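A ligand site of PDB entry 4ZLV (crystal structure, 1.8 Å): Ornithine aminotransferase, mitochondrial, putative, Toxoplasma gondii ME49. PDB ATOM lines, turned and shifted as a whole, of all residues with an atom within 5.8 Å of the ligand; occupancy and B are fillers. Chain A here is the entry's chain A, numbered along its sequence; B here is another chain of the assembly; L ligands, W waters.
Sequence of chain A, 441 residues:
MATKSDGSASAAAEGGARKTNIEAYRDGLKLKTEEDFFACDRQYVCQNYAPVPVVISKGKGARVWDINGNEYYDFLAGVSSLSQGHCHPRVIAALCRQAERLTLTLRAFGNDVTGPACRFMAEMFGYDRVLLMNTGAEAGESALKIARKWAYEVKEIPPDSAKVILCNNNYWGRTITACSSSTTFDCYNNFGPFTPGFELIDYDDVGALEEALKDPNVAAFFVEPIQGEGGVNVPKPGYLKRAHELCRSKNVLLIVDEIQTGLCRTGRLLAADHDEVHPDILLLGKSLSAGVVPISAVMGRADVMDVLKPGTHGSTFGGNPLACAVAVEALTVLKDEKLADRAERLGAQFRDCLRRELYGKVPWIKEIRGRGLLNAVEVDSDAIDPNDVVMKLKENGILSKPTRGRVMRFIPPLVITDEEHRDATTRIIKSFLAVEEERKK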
ATOM      1  N   VAL A  79     -26.043  15.733   6.467  1.00  0.00           N
ATOM      2  CA  VAL A  79     -25.198  15.717   7.665  1.00  0.00           C
ATOM      3  C   VAL A  79     -25.958  16.404   8.821  1.00  0.00           C
ATOM      4  O   VAL A  79     -25.469  17.366   9.476  1.00  0.00           O
ATOM      5  CB  VAL A  79     -23.798  16.335   7.429  1.00  0.00           C
ATOM      6  CG1 VAL A  79     -22.859  15.882   8.520  1.00  0.00           C
ATOM      7  CG2 VAL A  79     -23.192  15.941   6.061  1.00  0.00           C
ATOM      8  N   ASN A 134     -26.612  33.029   7.114  1.00  0.00           N
ATOM      9  CA  ASN A 134     -27.156  32.110   6.103  1.00  0.00           C
ATOM     10  C   ASN A 134     -26.537  30.729   6.252  1.00  0.00           C
ATOM     11  O   ASN A 134     -27.260  29.738   6.258  1.00  0.00           O
ATOM     12  CB  ASN A 134     -26.956  32.685   4.697  1.00  0.00           C
ATOM     13  CG  ASN A 134     -27.531  34.095   4.570  1.00  0.00           C
ATOM     14  OD1 ASN A 134     -28.723  34.284   4.421  1.00  0.00           O
ATOM     15  ND2 ASN A 134     -26.684  35.086   4.700  1.00  0.00           N
ATOM     16  N   THR A 135     -25.230  30.612   6.319  1.00  0.00           N
ATOM     17  CA  THR A 135     -24.596  29.289   6.349  1.00  0.00           C
ATOM     18  C   THR A 135     -23.948  29.039   7.698  1.00  0.00           C
ATOM     19  O   THR A 135     -23.752  29.971   8.461  1.00  0.00           O
ATOM     20  CB  THR A 135     -23.537  29.143   5.252  1.00  0.00           C
ATOM     21  OG1 THR A 135     -22.471  30.071   5.502  1.00  0.00           O
ATOM     22  CG2 THR A 135     -24.107  29.408   3.863  1.00  0.00           C
ATOM     23  N   GLY A 136     -23.581  27.782   7.958  1.00  0.00           N
ATOM     24  CA  GLY A 136     -22.893  27.459   9.202  1.00  0.00           C
ATOM     25  C   GLY A 136     -21.548  28.167   9.304  1.00  0.00           C
ATOM     26  O   GLY A 136     -21.205  28.728  10.359  1.00  0.00           O
ATOM     27  N   ALA A 137     -20.837  28.180   8.190  1.00  0.00           N
ATOM     28  CA  ALA A 137     -19.539  28.924   8.105  1.00  0.00           C
ATOM     29  C   ALA A 137     -19.692  30.385   8.495  1.00  0.00           C
ATOM     30  O   ALA A 137     -18.836  30.946   9.178  1.00  0.00           O
ATOM     31  CB  ALA A 137     -19.007  28.832   6.671  1.00  0.00           C
ATOM     32  N   GLU A 138     -20.721  31.029   7.984  1.00  0.00           N
ATOM     33  CA  GLU A 138     -20.986  32.449   8.313  1.00  0.00           C
ATOM     34  C   GLU A 138     -21.307  32.608   9.824  1.00  0.00           C
ATOM     35  O   GLU A 138     -20.934  33.625  10.408  1.00  0.00           O
ATOM     36  CB  GLU A 138     -22.131  33.043   7.501  1.00  0.00           C
ATOM     37  CG  GLU A 138     -21.801  33.301   6.051  1.00  0.00           C
ATOM     38  CD  GLU A 138     -22.923  34.046   5.342  1.00  0.00           C
ATOM     39  OE1 GLU A 138     -24.109  33.937   5.769  1.00  0.00           O
ATOM     40  OE2 GLU A 138     -22.587  34.786   4.400  1.00  0.00           O
ATOM     41  N   TYR A 171     -14.273  21.073  12.488  1.00  0.00           N
ATOM     42  CA  TYR A 171     -14.813  21.523  11.256  1.00  0.00           C
ATOM     43  C   TYR A 171     -15.840  22.568  11.508  1.00  0.00           C
ATOM     44  O   TYR A 171     -16.783  22.303  12.235  1.00  0.00           O
ATOM     45  CB  TYR A 171     -15.448  20.370  10.475  1.00  0.00           C
ATOM     46  CG  TYR A 171     -15.902  20.811   9.110  1.00  0.00           C
ATOM     47  CD1 TYR A 171     -14.976  20.960   8.086  1.00  0.00           C
ATOM     48  CD2 TYR A 171     -17.235  21.125   8.853  1.00  0.00           C
ATOM     49  CE1 TYR A 171     -15.352  21.394   6.824  1.00  0.00           C
ATOM     50  CE2 TYR A 171     -17.642  21.567   7.594  1.00  0.00           C
ATOM     51  CZ  TYR A 171     -16.697  21.680   6.585  1.00  0.00           C
ATOM     52  OH  TYR A 171     -17.047  22.119   5.309  1.00  0.00           O
ATOM     53  N   TRP A 172     -15.683  23.736  10.910  1.00  0.00           N
ATOM     54  CA  TRP A 172     -16.743  24.756  10.936  1.00  0.00           C
ATOM     55  C   TRP A 172     -16.979  25.470   9.623  1.00  0.00           C
ATOM     56  O   TRP A 172     -17.747  26.425   9.571  1.00  0.00           O
ATOM     57  CB  TRP A 172     -16.517  25.731  12.080  1.00  0.00           C
ATOM     58  CG  TRP A 172     -15.274  26.570  12.013  1.00  0.00           C
ATOM     59  CD1 TRP A 172     -14.053  26.241  12.519  1.00  0.00           C
ATOM     60  CD2 TRP A 172     -15.161  27.897  11.499  1.00  0.00           C
ATOM     61  NE1 TRP A 172     -13.162  27.273  12.279  1.00  0.00           N
ATOM     62  CE2 TRP A 172     -13.821  28.309  11.688  1.00  0.00           C
ATOM     63  CE3 TRP A 172     -16.038  28.755  10.825  1.00  0.00           C
ATOM     64  CZ2 TRP A 172     -13.365  29.562  11.294  1.00  0.00           C
ATOM     65  CZ3 TRP A 172     -15.570  30.006  10.425  1.00  0.00           C
ATOM     66  CH2 TRP A 172     -14.250  30.388  10.660  1.00  0.00           C
ATOM     67  N   GLY A 173     -16.424  24.951   8.530  1.00  0.00           N
ATOM     68  CA  GLY A 173     -16.694  25.507   7.226  1.00  0.00           C
ATOM     69  C   GLY A 173     -15.507  25.641   6.375  1.00  0.00           C
ATOM     70  O   GLY A 173     -14.454  25.081   6.677  1.00  0.00           O
ATOM     71  N   ARG A 174     -15.682  26.404   5.287  1.00  0.00           N
ATOM     72  CA  ARG A 174     -14.736  26.450   4.205  1.00  0.00           C
ATOM     73  C   ARG A 174     -14.212  27.839   3.853  1.00  0.00           C
ATOM     74  O   ARG A 174     -13.447  27.983   2.869  1.00  0.00           O
ATOM     75  CB  ARG A 174     -15.340  25.783   2.945  1.00  0.00           C
ATOM     76  CG  ARG A 174     -15.689  24.303   3.145  1.00  0.00           C
ATOM     77  CD  ARG A 174     -14.455  23.439   3.344  1.00  0.00           C
ATOM     78  NE  ARG A 174     -14.726  22.017   3.225  1.00  0.00           N
ATOM     79  CZ  ARG A 174     -13.885  21.086   2.779  1.00  0.00           C
ATOM     80  NH1 ARG A 174     -12.635  21.383   2.383  1.00  0.00           N
ATOM     81  NH2 ARG A 174     -14.301  19.828   2.728  1.00  0.00           N
ATOM     82  N   GLU A 224     -16.999  21.707  19.392  1.00  0.00           N
ATOM     83  CA  GLU A 224     -18.168  20.901  19.086  1.00  0.00           C
ATOM     84  C   GLU A 224     -18.436  19.919  20.259  1.00  0.00           C
ATOM     85  O   GLU A 224     -17.496  19.287  20.756  1.00  0.00           O
ATOM     86  CB  GLU A 224     -17.916  20.101  17.803  1.00  0.00           C
ATOM     87  CG  GLU A 224     -17.538  20.888  16.542  1.00  0.00           C
ATOM     88  CD  GLU A 224     -17.038  20.004  15.406  1.00  0.00           C
ATOM     89  OE1 GLU A 224     -17.880  19.273  14.744  1.00  0.00           O
ATOM     90  OE2 GLU A 224     -15.795  20.088  15.107  1.00  0.00           O
ATOM     91  N   GLY A 228     -18.061  16.371  14.414  1.00  0.00           N
ATOM     92  CA  GLY A 228     -18.903  15.817  13.361  1.00  0.00           C
ATOM     93  C   GLY A 228     -18.079  15.258  12.214  1.00  0.00           C
ATOM     94  O   GLY A 228     -17.867  14.027  12.114  1.00  0.00           O
ATOM     95  N   GLU A 229     -17.575  16.157  11.361  1.00  0.00           N
ATOM     96  CA  GLU A 229     -16.723  15.764  10.236  1.00  0.00           C
ATOM     97  C   GLU A 229     -15.483  15.063  10.698  1.00  0.00           C
ATOM     98  O   GLU A 229     -14.902  14.271   9.959  1.00  0.00           O
ATOM     99  CB  GLU A 229     -16.306  16.983   9.386  1.00  0.00           C
ATOM    100  CG  GLU A 229     -17.485  17.708   8.713  1.00  0.00           C
ATOM    101  CD  GLU A 229     -18.289  16.780   7.829  1.00  0.00           C
ATOM    102  OE1 GLU A 229     -17.702  16.308   6.818  1.00  0.00           O
ATOM    103  OE2 GLU A 229     -19.481  16.493   8.179  1.00  0.00           O
ATOM    104  N   ASP A 257     -20.431  25.077  18.954  1.00  0.00           N
ATOM    105  CA  ASP A 257     -20.962  24.843  17.607  1.00  0.00           C
ATOM    106  C   ASP A 257     -21.897  23.672  17.667  1.00  0.00           C
ATOM    107  O   ASP A 257     -21.455  22.543  17.774  1.00  0.00           O
ATOM    108  CB  ASP A 257     -19.800  24.569  16.639  1.00  0.00           C
ATOM    109  CG  ASP A 257     -20.270  24.483  15.207  1.00  0.00           C
ATOM    110  OD1 ASP A 257     -21.463  24.284  15.000  1.00  0.00           O
ATOM    111  OD2 ASP A 257     -19.435  24.616  14.273  1.00  0.00           O
ATOM    112  N   GLU A 258     -23.182  23.948  17.599  1.00  0.00           N
ATOM    113  CA  GLU A 258     -24.227  22.905  17.560  1.00  0.00           C
ATOM    114  C   GLU A 258     -24.899  22.842  16.189  1.00  0.00           C
ATOM    115  O   GLU A 258     -26.053  22.409  16.081  1.00  0.00           O
ATOM    116  CB  GLU A 258     -25.260  23.220  18.646  1.00  0.00           C
ATOM    117  CG  GLU A 258     -24.669  23.033  20.032  1.00  0.00           C
ATOM    118  CD  GLU A 258     -25.231  21.826  20.792  1.00  0.00           C
ATOM    119  OE1 GLU A 258     -25.791  20.849  20.148  1.00  0.00           O
ATOM    120  OE2 GLU A 258     -25.108  21.868  22.036  1.00  0.00           O
ATOM    121  N   ILE A 259     -24.170  23.278  15.150  1.00  0.00           N
ATOM    122  CA  ILE A 259     -24.693  23.261  13.788  1.00  0.00           C
ATOM    123  C   ILE A 259     -25.047  21.814  13.346  1.00  0.00           C
ATOM    124  O   ILE A 259     -26.059  21.571  12.648  1.00  0.00           O
ATOM    125  CB  ILE A 259     -23.721  23.971  12.829  1.00  0.00           C
ATOM    126  CG1 ILE A 259     -23.709  25.469  13.160  1.00  0.00           C
ATOM    127  CG2 ILE A 259     -24.106  23.742  11.377  1.00  0.00           C
ATOM    128  CD1 ILE A 259     -22.535  26.255  12.567  1.00  0.00           C
ATOM    129  N   GLN A 260     -24.223  20.866  13.766  1.00  0.00           N
ATOM    130  CA  GLN A 260     -24.479  19.433  13.495  1.00  0.00           C
ATOM    131  C   GLN A 260     -25.135  18.692  14.641  1.00  0.00           C
ATOM    132  O   GLN A 260     -26.013  17.860  14.423  1.00  0.00           O
ATOM    133  CB  GLN A 260     -23.197  18.724  13.057  1.00  0.00           C
ATOM    134  CG  GLN A 260     -23.452  17.278  12.569  1.00  0.00           C
ATOM    135  CD  GLN A 260     -22.236  16.634  11.919  1.00  0.00           C
ATOM    136  OE1 GLN A 260     -22.117  15.413  11.979  1.00  0.00           O
ATOM    137  NE2 GLN A 260     -21.367  17.427  11.275  1.00  0.00           N
ATOM    138  N   LYS A 286     -27.862  24.180   9.659  1.00  0.00           N
ATOM    139  CA  LYS A 286     -28.394  22.910   9.100  1.00  0.00           C
ATOM    140  C   LYS A 286     -29.916  22.697   9.280  1.00  0.00           C
ATOM    141  O   LYS A 286     -30.697  23.397   8.609  1.00  0.00           O
ATOM    142  CB  LYS A 286     -27.504  21.774   9.606  1.00  0.00           C
ATOM    143  CG  LYS A 286     -26.110  21.789   8.943  1.00  0.00           C
ATOM    144  CD  LYS A 286     -25.321  20.513   9.202  1.00  0.00           C
ATOM    145  CE  LYS A 286     -24.074  20.343   8.341  1.00  0.00           C
ATOM    146  NZ  LYS A 286     -22.870  21.069   8.758  1.00  0.00           N
ATOM    147  N   GLU B 138     -19.433  34.167   0.405  1.00  0.00           N
ATOM    148  CA  GLU B 138     -18.905  32.813   0.117  1.00  0.00           C
ATOM    149  C   GLU B 138     -18.338  32.691  -1.318  1.00  0.00           C
ATOM    150  O   GLU B 138     -17.346  31.996  -1.573  1.00  0.00           O
ATOM    151  CB  GLU B 138     -20.015  31.765   0.319  1.00  0.00           C
ATOM    152  CG  GLU B 138     -20.135  31.313   1.749  1.00  0.00           C
ATOM    153  CD  GLU B 138     -21.202  30.246   1.931  1.00  0.00           C
ATOM    154  OE1 GLU B 138     -21.975  29.999   0.965  1.00  0.00           O
ATOM    155  OE2 GLU B 138     -21.233  29.697   3.041  1.00  0.00           O
ATOM    156  N   SER B 315     -19.659  22.951   0.840  1.00  0.00           N
ATOM    157  CA  SER B 315     -20.688  23.749   1.461  1.00  0.00           C
ATOM    158  C   SER B 315     -21.909  22.876   1.616  1.00  0.00           C
ATOM    159  O   SER B 315     -22.302  22.203   0.681  1.00  0.00           O
ATOM    160  CB  SER B 315     -21.062  24.938   0.545  1.00  0.00           C
ATOM    161  OG  SER B 315     -22.201  25.597   1.040  1.00  0.00           O
ATOM    162  N   THR B 316     -22.571  22.975   2.735  1.00  0.00           N
ATOM    163  CA  THR B 316     -23.792  22.138   2.963  1.00  0.00           C
ATOM    164  C   THR B 316     -24.847  22.472   1.912  1.00  0.00           C
ATOM    165  O   THR B 316     -25.297  21.588   1.186  1.00  0.00           O
ATOM    166  CB  THR B 316     -24.354  22.291   4.369  1.00  0.00           C
ATOM    167  OG1 THR B 316     -23.371  21.831   5.285  1.00  0.00           O
ATOM    168  CG2 THR B 316     -25.651  21.477   4.546  1.00  0.00           C
ATOM    169  N   PHE B 317     -25.247  23.730   1.860  1.00  0.00           N
ATOM    170  CA  PHE B 317     -26.365  24.148   0.969  1.00  0.00           C
ATOM    171  C   PHE B 317     -25.979  24.584  -0.431  1.00  0.00           C
ATOM    172  O   PHE B 317     -26.845  24.821  -1.247  1.00  0.00           O
ATOM    173  CB  PHE B 317     -27.180  25.281   1.643  1.00  0.00           C
ATOM    174  CG  PHE B 317     -28.069  24.796   2.753  1.00  0.00           C
ATOM    175  CD1 PHE B 317     -27.583  24.696   4.019  1.00  0.00           C
ATOM    176  CD2 PHE B 317     -29.356  24.406   2.506  1.00  0.00           C
ATOM    177  CE1 PHE B 317     -28.385  24.217   5.048  1.00  0.00           C
ATOM    178  CE2 PHE B 317     -30.148  23.896   3.507  1.00  0.00           C
ATOM    179  CZ  PHE B 317     -29.672  23.827   4.802  1.00  0.00           C
HETATM  180  N1  LIG L   1     -19.972  23.503  11.853  1.00  0.00           N
HETATM  181  C1  LIG L   1     -20.319  22.193  11.974  1.00  0.00           C
HETATM  182  C2  LIG L   1     -20.130  21.469  13.294  1.00  0.00           C
HETATM  183  C3  LIG L   1     -20.860  21.462  10.812  1.00  0.00           C
HETATM  184  O1  LIG L   1     -21.188  20.153  10.866  1.00  0.00           O
HETATM  185  C4  LIG L   1     -21.037  22.189   9.536  1.00  0.00           C
HETATM  186  C5  LIG L   1     -21.638  21.418   8.399  1.00  0.00           C
HETATM  187  C6  LIG L   1     -20.613  23.616   9.521  1.00  0.00           C
HETATM  188  C7  LIG L   1     -20.098  24.177  10.693  1.00  0.00           C
HETATM  189  C8  LIG L   1     -20.666  24.486   8.281  1.00  0.00           C
HETATM  190  O2  LIG L   1     -21.948  24.782   7.851  1.00  0.00           O
HETATM  191  P1  LIG L   1     -22.174  25.141   6.307  1.00  0.00           P
HETATM  192  O3  LIG L   1     -21.823  23.926   5.488  1.00  0.00           O
HETATM  193  O4  LIG L   1     -21.178  26.253   6.035  1.00  0.00           O
HETATM  194  O5  LIG L   1     -23.608  25.569   6.347  1.00  0.00           O
HETATM  195  O   HOH W   1     -24.336  25.868   3.643  1.00  0.00           O
HETATM  196  O   HOH W   2     -18.716  25.992   4.595  1.00  0.00           O
HETATM  197  O   HOH W   3     -22.242  20.566  15.923  1.00  0.00           O
HETATM  198  O   HOH W   4     -21.716  27.058   3.277  1.00  0.00           O
HETATM  199  O   HOH W   5     -25.835  25.316   8.202  1.00  0.00           O
HETATM  200  O   HOH W   6     -20.266  18.760  15.351  1.00  0.00           O
HETATM  201  O   HOH W   7     -18.435  18.796  11.813  1.00  0.00           O
HETATM  202  O   HOH W   8     -19.361  23.138   4.660  1.00  0.00           O
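The backbone NH (N) of Ile 259 sits at hydrogen-bond distance from the side-chain carboxylate (OD1) of Asp 257, at 2.9 Å. The side-chain carboxylate (OE2) of Glu 224 is in hydrogen-bond range of the backbone NH (N) of Tyr 171. OH of Tyr 171 lies within hydrogen-bond range of NE of Arg 174 (3.1 Å). OE1 of Glu 224 lies within hydrogen-bond range of N of Gly 228, 2.9 Å away. The side-chain carboxylate (OE2) of Glu 138 of chain B lies within hydrogen-bond range of the side-chain hydroxyl (OG1) of Thr 135. N of Glu 138 of chain A is in hydrogen-bond range of OG1 of Thr 135.
A carbon (C5) of the ligand is covalently linked to the side-chain amino group (NZ) of Lys 286 (1.3 Å). N of Thr 316 of chain B lies within hydrogen-bond range of O3 of the ligand. OG1 of Thr 316 of chain B lies within hydrogen-bond range of O3 of the ligand (2.6 Å). The side-chain carboxylate (OD2) of Asp 257 is in hydrogen-bond range of a nitrogen (N1) of the ligand, at 2.7 Å. The backbone NH of Gly 136 is in hydrogen-bond range of an oxygen (O5) of the ligand (2.7 Å). NE2 of Gln 260 lies within hydrogen-bond range of O1 of the ligand (2.8 Å). An oxygen (O4) of the ligand is in hydrogen-bond range of the backbone NH (N) of Ala 137.
Water W8 lies within hydrogen-bond range of OH of Tyr 171 and O3 of the ligand. Water W1 lies within hydrogen-bond range of an oxygen (O5) of the ligand (2.8 Å), the backbone NH of Phe 317 of chain B (2.9 Å) and the side-chain hydroxyl of Ser 315 of chain B (3.4 Å). Water W2 lies within hydrogen-bond range of O4 of the ligand (2.9 Å) and N of Arg 174 (3.1 Å). Water W5 lies within hydrogen-bond range of the backbone NH of Lys 286 (2.7 Å), an oxygen (O5) of the ligand (2.9 Å) and the backbone NH of Gly 136 (3.3 Å). Water W4 lies within hydrogen-bond range of OE2 of Glu 138 of chain B (2.7 Å), OG of Ser 315 of chain B (2.7 Å) and O4 of the ligand (2.9 Å). Water W6 lies within hydrogen-bond range of the side-chain carboxylate (OE1) of Glu 224 (2.5 Å) and the backbone NH (N) of Gly 228 (3.4 Å).
A nitrogen (N1) of the ligand sits close to the backbone carbonyl oxygen (O) of Tyr 171 (3.4 Å). Residues that only touch the ligand: Trp 172, Glu 224, Ile 259 and Thr 135. Hydrophobic or aromatic side chains within 4 Å of the ligand: Ala 137, Tyr 171 and Ile 259. 11 residues have an atom within 4 Å of the ligand: Thr 135, Gly 136, Ala 137, Tyr 171, Trp 172, Glu 224, Asp 257, Ile 259, Gln 260, Lys 286 and Thr 316 of chain B. The nearest printed residue that does not touch the ligand is Ser 315 of chain B (4.01 Å).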
